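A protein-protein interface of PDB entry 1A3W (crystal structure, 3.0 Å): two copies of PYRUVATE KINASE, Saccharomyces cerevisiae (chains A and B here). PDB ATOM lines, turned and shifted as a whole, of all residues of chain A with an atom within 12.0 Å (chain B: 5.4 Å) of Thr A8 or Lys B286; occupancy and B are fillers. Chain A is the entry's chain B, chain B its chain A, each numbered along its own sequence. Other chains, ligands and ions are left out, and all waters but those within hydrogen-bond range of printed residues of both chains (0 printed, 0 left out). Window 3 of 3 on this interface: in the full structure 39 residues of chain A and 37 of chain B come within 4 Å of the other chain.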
ATOM      1  N   SER A   2      -8.030  26.877 -14.131  1.00  0.00           N
ATOM      2  CA  SER A   2      -7.701  26.596 -12.703  1.00  0.00           C
ATOM      3  C   SER A   2      -6.419  25.784 -12.590  1.00  0.00           C
ATOM      4  O   SER A   2      -5.345  26.338 -12.349  1.00  0.00           O
ATOM      5  CB  SER A   2      -8.845  25.836 -12.033  1.00  0.00           C
ATOM      6  OG  SER A   2      -8.759  25.933 -10.621  1.00  0.00           O
ATOM      7  N   ARG A   3      -6.535  24.470 -12.763  1.00  0.00           N
ATOM      8  CA  ARG A   3      -5.379  23.584 -12.680  1.00  0.00           C
ATOM      9  C   ARG A   3      -4.351  23.975 -13.734  1.00  0.00           C
ATOM     10  O   ARG A   3      -3.144  23.958 -13.478  1.00  0.00           O
ATOM     11  CB  ARG A   3      -5.814  22.130 -12.884  1.00  0.00           C
ATOM     12  CG  ARG A   3      -4.714  21.205 -13.373  1.00  0.00           C
ATOM     13  CD  ARG A   3      -5.288  20.112 -14.256  1.00  0.00           C
ATOM     14  NE  ARG A   3      -4.494  19.916 -15.465  1.00  0.00           N
ATOM     15  CZ  ARG A   3      -3.485  19.056 -15.559  1.00  0.00           C
ATOM     16  NH1 ARG A   3      -3.155  18.317 -14.513  1.00  0.00           N
ATOM     17  NH2 ARG A   3      -2.810  18.936 -16.696  1.00  0.00           N
ATOM     18  N   LEU A   4      -4.841  24.332 -14.917  1.00  0.00           N
ATOM     19  CA  LEU A   4      -3.972  24.730 -16.016  1.00  0.00           C
ATOM     20  C   LEU A   4      -3.251  26.044 -15.721  1.00  0.00           C
ATOM     21  O   LEU A   4      -2.052  26.174 -15.965  1.00  0.00           O
ATOM     22  CB  LEU A   4      -4.790  24.864 -17.304  1.00  0.00           C
ATOM     23  CG  LEU A   4      -4.592  23.797 -18.389  1.00  0.00           C
ATOM     24  CD1 LEU A   4      -3.103  23.492 -18.559  1.00  0.00           C
ATOM     25  CD2 LEU A   4      -5.367  22.539 -18.016  1.00  0.00           C
ATOM     26  N   GLU A   5      -3.990  27.017 -15.195  1.00  0.00           N
ATOM     27  CA  GLU A   5      -3.421  28.314 -14.862  1.00  0.00           C
ATOM     28  C   GLU A   5      -2.318  28.142 -13.832  1.00  0.00           C
ATOM     29  O   GLU A   5      -1.194  28.595 -14.033  1.00  0.00           O
ATOM     30  CB  GLU A   5      -4.500  29.246 -14.310  1.00  0.00           C
ATOM     31  CG  GLU A   5      -4.372  30.688 -14.786  1.00  0.00           C
ATOM     32  CD  GLU A   5      -4.971  31.686 -13.810  1.00  0.00           C
ATOM     33  OE1 GLU A   5      -5.976  31.346 -13.149  1.00  0.00           O
ATOM     34  OE2 GLU A   5      -4.435  32.811 -13.705  1.00  0.00           O
ATOM     35  N   ARG A   6      -2.649  27.481 -12.727  1.00  0.00           N
ATOM     36  CA  ARG A   6      -1.687  27.237 -11.659  1.00  0.00           C
ATOM     37  C   ARG A   6      -0.465  26.505 -12.200  1.00  0.00           C
ATOM     38  O   ARG A   6       0.662  26.969 -12.053  1.00  0.00           O
ATOM     39  CB  ARG A   6      -2.332  26.403 -10.551  1.00  0.00           C
ATOM     40  CG  ARG A   6      -1.337  25.705  -9.642  1.00  0.00           C
ATOM     41  CD  ARG A   6      -2.038  24.789  -8.655  1.00  0.00           C
ATOM     42  NE  ARG A   6      -1.459  23.449  -8.658  1.00  0.00           N
ATOM     43  CZ  ARG A   6      -2.111  22.359  -9.049  1.00  0.00           C
ATOM     44  NH1 ARG A   6      -3.368  22.452  -9.467  1.00  0.00           N
ATOM     45  NH2 ARG A   6      -1.509  21.174  -9.021  1.00  0.00           N
ATOM     46  N   LEU A   7      -0.703  25.360 -12.829  1.00  0.00           N
ATOM     47  CA  LEU A   7       0.374  24.559 -13.390  1.00  0.00           C
ATOM     48  C   LEU A   7       1.221  25.390 -14.333  1.00  0.00           C
ATOM     49  O   LEU A   7       2.438  25.228 -14.403  1.00  0.00           O
ATOM     50  CB  LEU A   7      -0.198  23.359 -14.145  1.00  0.00           C
ATOM     51  CG  LEU A   7      -0.173  22.013 -13.414  1.00  0.00           C
ATOM     52  CD1 LEU A   7      -0.972  22.111 -12.129  1.00  0.00           C
ATOM     53  CD2 LEU A   7      -0.751  20.934 -14.313  1.00  0.00           C
ATOM     54  N   THR A   8       0.563  26.276 -15.068  1.00  0.00           N
ATOM     55  CA  THR A   8       1.257  27.135 -16.011  1.00  0.00           C
ATOM     56  C   THR A   8       2.187  28.061 -15.247  1.00  0.00           C
ATOM     57  O   THR A   8       3.281  28.382 -15.709  1.00  0.00           O
ATOM     58  CB  THR A   8       0.270  27.993 -16.817  1.00  0.00           C
ATOM     59  OG1 THR A   8      -0.629  27.145 -17.542  1.00  0.00           O
ATOM     60  CG2 THR A   8       1.026  28.880 -17.797  1.00  0.00           C
ATOM     61  N   SER A   9       1.741  28.481 -14.067  1.00  0.00           N
ATOM     62  CA  SER A   9       2.515  29.381 -13.224  1.00  0.00           C
ATOM     63  C   SER A   9       3.028  28.692 -11.967  1.00  0.00           C
ATOM     64  O   SER A   9       2.343  28.659 -10.944  1.00  0.00           O
ATOM     65  CB  SER A   9       1.662  30.587 -12.828  1.00  0.00           C
ATOM     66  OG  SER A   9       0.481  30.649 -13.606  1.00  0.00           O
ATOM     67  N   LEU A  10       4.235  28.142 -12.049  1.00  0.00           N
ATOM     68  CA  LEU A  10       4.850  27.467 -10.914  1.00  0.00           C
ATOM     69  C   LEU A  10       6.143  28.194 -10.546  1.00  0.00           C
ATOM     70  O   LEU A  10       6.498  28.228  -9.344  1.00  0.00           O
ATOM     71  CB  LEU A  10       5.148  26.002 -11.263  1.00  0.00           C
ATOM     72  CG  LEU A  10       4.251  24.946 -10.600  1.00  0.00           C
ATOM     73  CD1 LEU A  10       2.807  25.161 -11.012  1.00  0.00           C
ATOM     74  CD2 LEU A  10       4.703  23.556 -10.994  1.00  0.00           C
ATOM     75  N   LEU A 323       2.644  15.354  -3.578  1.00  0.00           N
ATOM     76  CA  LEU A 323       1.561  16.060  -4.264  1.00  0.00           C
ATOM     77  C   LEU A 323       0.266  15.262  -4.313  1.00  0.00           C
ATOM     78  O   LEU A 323      -0.800  15.831  -4.512  1.00  0.00           O
ATOM     79  CB  LEU A 323       1.975  16.431  -5.690  1.00  0.00           C
ATOM     80  CG  LEU A 323       2.738  17.748  -5.798  1.00  0.00           C
ATOM     81  CD1 LEU A 323       3.574  17.778  -7.059  1.00  0.00           C
ATOM     82  CD2 LEU A 323       1.751  18.889  -5.780  1.00  0.00           C
ATOM     83  N   GLN A 357       5.245  23.031  -2.642  1.00  0.00           N
ATOM     84  CA  GLN A 357       5.326  24.424  -3.061  1.00  0.00           C
ATOM     85  C   GLN A 357       4.462  24.643  -4.300  1.00  0.00           C
ATOM     86  O   GLN A 357       4.143  25.775  -4.657  1.00  0.00           O
ATOM     87  CB  GLN A 357       6.775  24.792  -3.377  1.00  0.00           C
ATOM     88  CG  GLN A 357       7.210  26.132  -2.816  1.00  0.00           C
ATOM     89  CD  GLN A 357       8.615  26.097  -2.244  1.00  0.00           C
ATOM     90  OE1 GLN A 357       8.856  25.488  -1.199  1.00  0.00           O
ATOM     91  NE2 GLN A 357       9.552  26.751  -2.927  1.00  0.00           N
ATOM     92  N   ALA A 358       4.089  23.545  -4.948  1.00  0.00           N
ATOM     93  CA  ALA A 358       3.275  23.598  -6.149  1.00  0.00           C
ATOM     94  C   ALA A 358       1.937  22.929  -5.899  1.00  0.00           C
ATOM     95  O   ALA A 358       1.406  22.250  -6.774  1.00  0.00           O
ATOM     96  CB  ALA A 358       3.996  22.909  -7.301  1.00  0.00           C
ATOM     97  N   ILE A 359       1.392  23.120  -4.704  1.00  0.00           N
ATOM     98  CA  ILE A 359       0.106  22.523  -4.362  1.00  0.00           C
ATOM     99  C   ILE A 359      -1.005  23.568  -4.379  1.00  0.00           C
ATOM    100  O   ILE A 359      -0.751  24.756  -4.185  1.00  0.00           O
ATOM    101  CB  ILE A 359       0.137  21.880  -2.960  1.00  0.00           C
ATOM    102  CG1 ILE A 359       1.217  20.800  -2.903  1.00  0.00           C
ATOM    103  CG2 ILE A 359      -1.225  21.287  -2.627  1.00  0.00           C
ATOM    104  CD1 ILE A 359       1.113  19.889  -1.688  1.00  0.00           C
ATOM    105  N   ALA A 360      -2.231  23.114  -4.620  1.00  0.00           N
ATOM    106  CA  ALA A 360      -3.394  23.994  -4.648  1.00  0.00           C
ATOM    107  C   ALA A 360      -4.094  23.885  -3.297  1.00  0.00           C
ATOM    108  O   ALA A 360      -4.931  23.009  -3.091  1.00  0.00           O
ATOM    109  CB  ALA A 360      -4.335  23.577  -5.764  1.00  0.00           C
ATOM    110  N   PHE B 250      11.670  29.908 -22.821  1.00  0.00           N
ATOM    111  CA  PHE B 250      10.892  28.784 -23.328  1.00  0.00           C
ATOM    112  C   PHE B 250       9.550  29.242 -23.875  1.00  0.00           C
ATOM    113  O   PHE B 250       8.882  28.498 -24.589  1.00  0.00           O
ATOM    114  CB  PHE B 250      10.636  27.749 -22.229  1.00  0.00           C
ATOM    115  CG  PHE B 250       9.482  26.838 -22.530  1.00  0.00           C
ATOM    116  CD1 PHE B 250       9.652  25.732 -23.350  1.00  0.00           C
ATOM    117  CD2 PHE B 250       8.214  27.109 -22.031  1.00  0.00           C
ATOM    118  CE1 PHE B 250       8.578  24.912 -23.676  1.00  0.00           C
ATOM    119  CE2 PHE B 250       7.133  26.296 -22.350  1.00  0.00           C
ATOM    120  CZ  PHE B 250       7.316  25.193 -23.175  1.00  0.00           C
ATOM    121  N   ASP B 251       9.142  30.454 -23.523  1.00  0.00           N
ATOM    122  CA  ASP B 251       7.864  30.959 -23.995  1.00  0.00           C
ATOM    123  C   ASP B 251       7.945  31.405 -25.445  1.00  0.00           C
ATOM    124  O   ASP B 251       7.114  31.017 -26.268  1.00  0.00           O
ATOM    125  CB  ASP B 251       7.392  32.097 -23.101  1.00  0.00           C
ATOM    126  CG  ASP B 251       6.645  31.592 -21.889  1.00  0.00           C
ATOM    127  OD1 ASP B 251       5.856  30.631 -22.047  1.00  0.00           O
ATOM    128  OD2 ASP B 251       6.852  32.149 -20.785  1.00  0.00           O
ATOM    129  N   LEU B 254       8.501  28.236 -27.381  1.00  0.00           N
ATOM    130  CA  LEU B 254       7.249  27.519 -27.527  1.00  0.00           C
ATOM    131  C   LEU B 254       6.429  28.030 -28.720  1.00  0.00           C
ATOM    132  O   LEU B 254       5.694  27.275 -29.349  1.00  0.00           O
ATOM    133  CB  LEU B 254       6.445  27.670 -26.239  1.00  0.00           C
ATOM    134  CG  LEU B 254       5.461  26.566 -25.845  1.00  0.00           C
ATOM    135  CD1 LEU B 254       4.079  27.159 -25.799  1.00  0.00           C
ATOM    136  CD2 LEU B 254       5.502  25.389 -26.815  1.00  0.00           C
ATOM    137  N   LYS B 281       6.179  19.696 -14.855  1.00  0.00           N
ATOM    138  CA  LYS B 281       4.754  19.993 -14.722  1.00  0.00           C
ATOM    139  C   LYS B 281       4.350  21.290 -15.397  1.00  0.00           C
ATOM    140  O   LYS B 281       3.254  21.393 -15.950  1.00  0.00           O
ATOM    141  CB  LYS B 281       4.367  20.060 -13.246  1.00  0.00           C
ATOM    142  CG  LYS B 281       4.346  18.715 -12.556  1.00  0.00           C
ATOM    143  CD  LYS B 281       4.023  18.856 -11.084  1.00  0.00           C
ATOM    144  CE  LYS B 281       3.366  17.596 -10.554  1.00  0.00           C
ATOM    145  NZ  LYS B 281       3.644  16.416 -11.418  1.00  0.00           N
ATOM    146  N   LYS B 282       5.237  22.281 -15.350  1.00  0.00           N
ATOM    147  CA  LYS B 282       4.963  23.577 -15.961  1.00  0.00           C
ATOM    148  C   LYS B 282       5.058  23.522 -17.483  1.00  0.00           C
ATOM    149  O   LYS B 282       4.078  23.786 -18.179  1.00  0.00           O
ATOM    150  CB  LYS B 282       5.927  24.633 -15.425  1.00  0.00           C
ATOM    151  CG  LYS B 282       5.260  25.957 -15.117  1.00  0.00           C
ATOM    152  CD  LYS B 282       6.125  27.115 -15.560  1.00  0.00           C
ATOM    153  CE  LYS B 282       6.088  28.245 -14.546  1.00  0.00           C
ATOM    154  NZ  LYS B 282       6.227  29.580 -15.196  1.00  0.00           N
ATOM    155  N   LEU B 283       6.238  23.180 -17.993  1.00  0.00           N
ATOM    156  CA  LEU B 283       6.458  23.088 -19.434  1.00  0.00           C
ATOM    157  C   LEU B 283       5.409  22.206 -20.099  1.00  0.00           C
ATOM    158  O   LEU B 283       4.745  22.630 -21.046  1.00  0.00           O
ATOM    159  CB  LEU B 283       7.854  22.537 -19.720  1.00  0.00           C
ATOM    160  CG  LEU B 283       8.967  23.582 -19.853  1.00  0.00           C
ATOM    161  CD1 LEU B 283       8.752  24.705 -18.855  1.00  0.00           C
ATOM    162  CD2 LEU B 283      10.322  22.930 -19.621  1.00  0.00           C
ATOM    163  N   ILE B 284       5.257  20.982 -19.603  1.00  0.00           N
ATOM    164  CA  ILE B 284       4.270  20.055 -20.145  1.00  0.00           C
ATOM    165  C   ILE B 284       2.901  20.730 -20.225  1.00  0.00           C
ATOM    166  O   ILE B 284       2.162  20.543 -21.194  1.00  0.00           O
ATOM    167  CB  ILE B 284       4.143  18.793 -19.264  1.00  0.00           C
ATOM    168  CG1 ILE B 284       5.139  17.733 -19.733  1.00  0.00           C
ATOM    169  CG2 ILE B 284       2.718  18.246 -19.318  1.00  0.00           C
ATOM    170  CD1 ILE B 284       4.882  16.351 -19.167  1.00  0.00           C
ATOM    171  N   ALA B 285       2.570  21.512 -19.202  1.00  0.00           N
ATOM    172  CA  ALA B 285       1.290  22.213 -19.145  1.00  0.00           C
ATOM    173  C   ALA B 285       1.255  23.418 -20.079  1.00  0.00           C
ATOM    174  O   ALA B 285       0.238  23.700 -20.706  1.00  0.00           O
ATOM    175  CB  ALA B 285       1.012  22.658 -17.717  1.00  0.00           C
ATOM    176  N   LYS B 286       2.372  24.132 -20.156  1.00  0.00           N
ATOM    177  CA  LYS B 286       2.478  25.304 -21.010  1.00  0.00           C
ATOM    178  C   LYS B 286       2.385  24.877 -22.467  1.00  0.00           C
ATOM    179  O   LYS B 286       2.096  25.692 -23.345  1.00  0.00           O
ATOM    180  CB  LYS B 286       3.812  26.013 -20.775  1.00  0.00           C
ATOM    181  CG  LYS B 286       3.762  27.106 -19.723  1.00  0.00           C
ATOM    182  CD  LYS B 286       4.653  28.276 -20.108  1.00  0.00           C
ATOM    183  CE  LYS B 286       4.874  29.217 -18.933  1.00  0.00           C
ATOM    184  NZ  LYS B 286       6.249  29.796 -18.938  1.00  0.00           N
ATOM    185  N   SER B 287       2.634  23.596 -22.719  1.00  0.00           N
ATOM    186  CA  SER B 287       2.580  23.062 -24.071  1.00  0.00           C
ATOM    187  C   SER B 287       1.177  22.619 -24.452  1.00  0.00           C
ATOM    188  O   SER B 287       0.733  22.859 -25.573  1.00  0.00           O
ATOM    189  CB  SER B 287       3.549  21.897 -24.211  1.00  0.00           C
ATOM    190  OG  SER B 287       4.876  22.348 -24.004  1.00  0.00           O
ATOM    191  N   ASN B 288       0.477  21.972 -23.526  1.00  0.00           N
ATOM    192  CA  ASN B 288      -0.886  21.527 -23.794  1.00  0.00           C
ATOM    193  C   ASN B 288      -1.706  22.748 -24.185  1.00  0.00           C
ATOM    194  O   ASN B 288      -2.518  22.705 -25.111  1.00  0.00           O
ATOM    195  CB  ASN B 288      -1.496  20.877 -22.553  1.00  0.00           C
ATOM    196  CG  ASN B 288      -0.927  19.505 -22.276  1.00  0.00           C
ATOM    197  OD1 ASN B 288      -0.247  18.921 -23.116  1.00  0.00           O
ATOM    198  ND2 ASN B 288      -1.205  18.983 -21.093  1.00  0.00           N
ATOM    199  N   LEU B 289      -1.478  23.840 -23.467  1.00  0.00           N
ATOM    200  CA  LEU B 289      -2.168  25.095 -23.719  1.00  0.00           C
ATOM    201  C   LEU B 289      -1.920  25.547 -25.158  1.00  0.00           C
ATOM    202  O   LEU B 289      -2.860  25.772 -25.919  1.00  0.00           O
ATOM    203  CB  LEU B 289      -1.661  26.166 -22.750  1.00  0.00           C
ATOM    204  CG  LEU B 289      -2.469  27.457 -22.626  1.00  0.00           C
ATOM    205  CD1 LEU B 289      -3.707  27.223 -21.770  1.00  0.00           C
ATOM    206  CD2 LEU B 289      -1.583  28.535 -22.019  1.00  0.00           C
ATOM    207  N   ALA B 290      -0.646  25.672 -25.521  1.00  0.00           N
ATOM    208  CA  ALA B 290      -0.257  26.102 -26.858  1.00  0.00           C
ATOM    209  C   ALA B 290      -0.711  25.127 -27.929  1.00  0.00           C
ATOM    210  O   ALA B 290      -0.776  25.480 -29.107  1.00  0.00           O
ATOM    211  CB  ALA B 290       1.244  26.278 -26.929  1.00  0.00           C
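The side-chain amino group of Lys B282 lies close to the backbone carbonyl oxygen of Thr A8, 3.2 Å away.
Among the printed residues, merely in contact across the chains: Leu A4 with Ala B285, Leu A7 with Lys B282, Leu A7 with Ala B285, Thr A8 with Lys B286, Ser A9 with Lys B282, Leu A10 with Lys B282 and Leu A323 with Lys B281.
The backbone carbonyl oxygen of Glu A5 is in hydrogen-bond range of the side-chain hydroxyl of Ser A9. NZ of Lys B286 is in salt-bridge range of OD2 of Asp B251 (3.1 Å).
Of the 13 printed residues of chain B, 4 touch a printed residue of chain A. Printed residues of chain B that touch a printed residue of chain A: Lys B281, Lys B282, Ala B285 and Lys B286. Hydrophobic or aromatic side chains of chain B within 4 Å of the printed part of chain A: Ala B285. Of the 14 printed residues of chain A, 6 touch a printed residue of chain B. Hydrophobic or aromatic side chains of chain A within 4 Å of the printed part of chain B: Leu A4, Leu A7, Leu A10 and Leu A323. Among the printed residues, 8 pairs touch across the chains. Among the printed residues, no Asp or Glu carboxylate lies within 4 Å of a Lys or Arg side-chain nitrogen of the other chain.
No position is printed for both chains.
Arg A3 touches none of the printed residues of chain B. Printed residues of chain B within 4 Å of Leu A4: Ala B285. Printed residues of chain B within 4 Å of Leu A7: Lys B282 and Ala B285. Of chain B, only Lys B282 and Lys B286 come within 4 Å of Thr A8. Of the printed residues of chain B, Leu A10 touches Lys B282 (3.1 Å). Of the printed residues of chain B, Leu A323 touches Lys B281. Phe B250 touches none of the printed residues of chain A. No residue of chain A comes within 4 Å of Asp B251. Printed residues of chain A within 4 Å of Lys B281: Leu A323. No residue of chain A comes within 4 Å of Leu B283. Of chain A, only Leu A4 and Leu A7 come within 4 Å of Ala B285. Of the printed residues of chain A, Lys B286 touches Thr A8 (3.7 Å). Leu B289 touches none of the printed residues of chain A. No residue of chain A comes within 4 Å of Ala B290. The nearest residue of chain A that does not touch Lys B286 is Leu A4 (5.7 Å). The nearest printed residue of chain B that does not touch Leu A7 is Lys B281 (4.2 Å).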
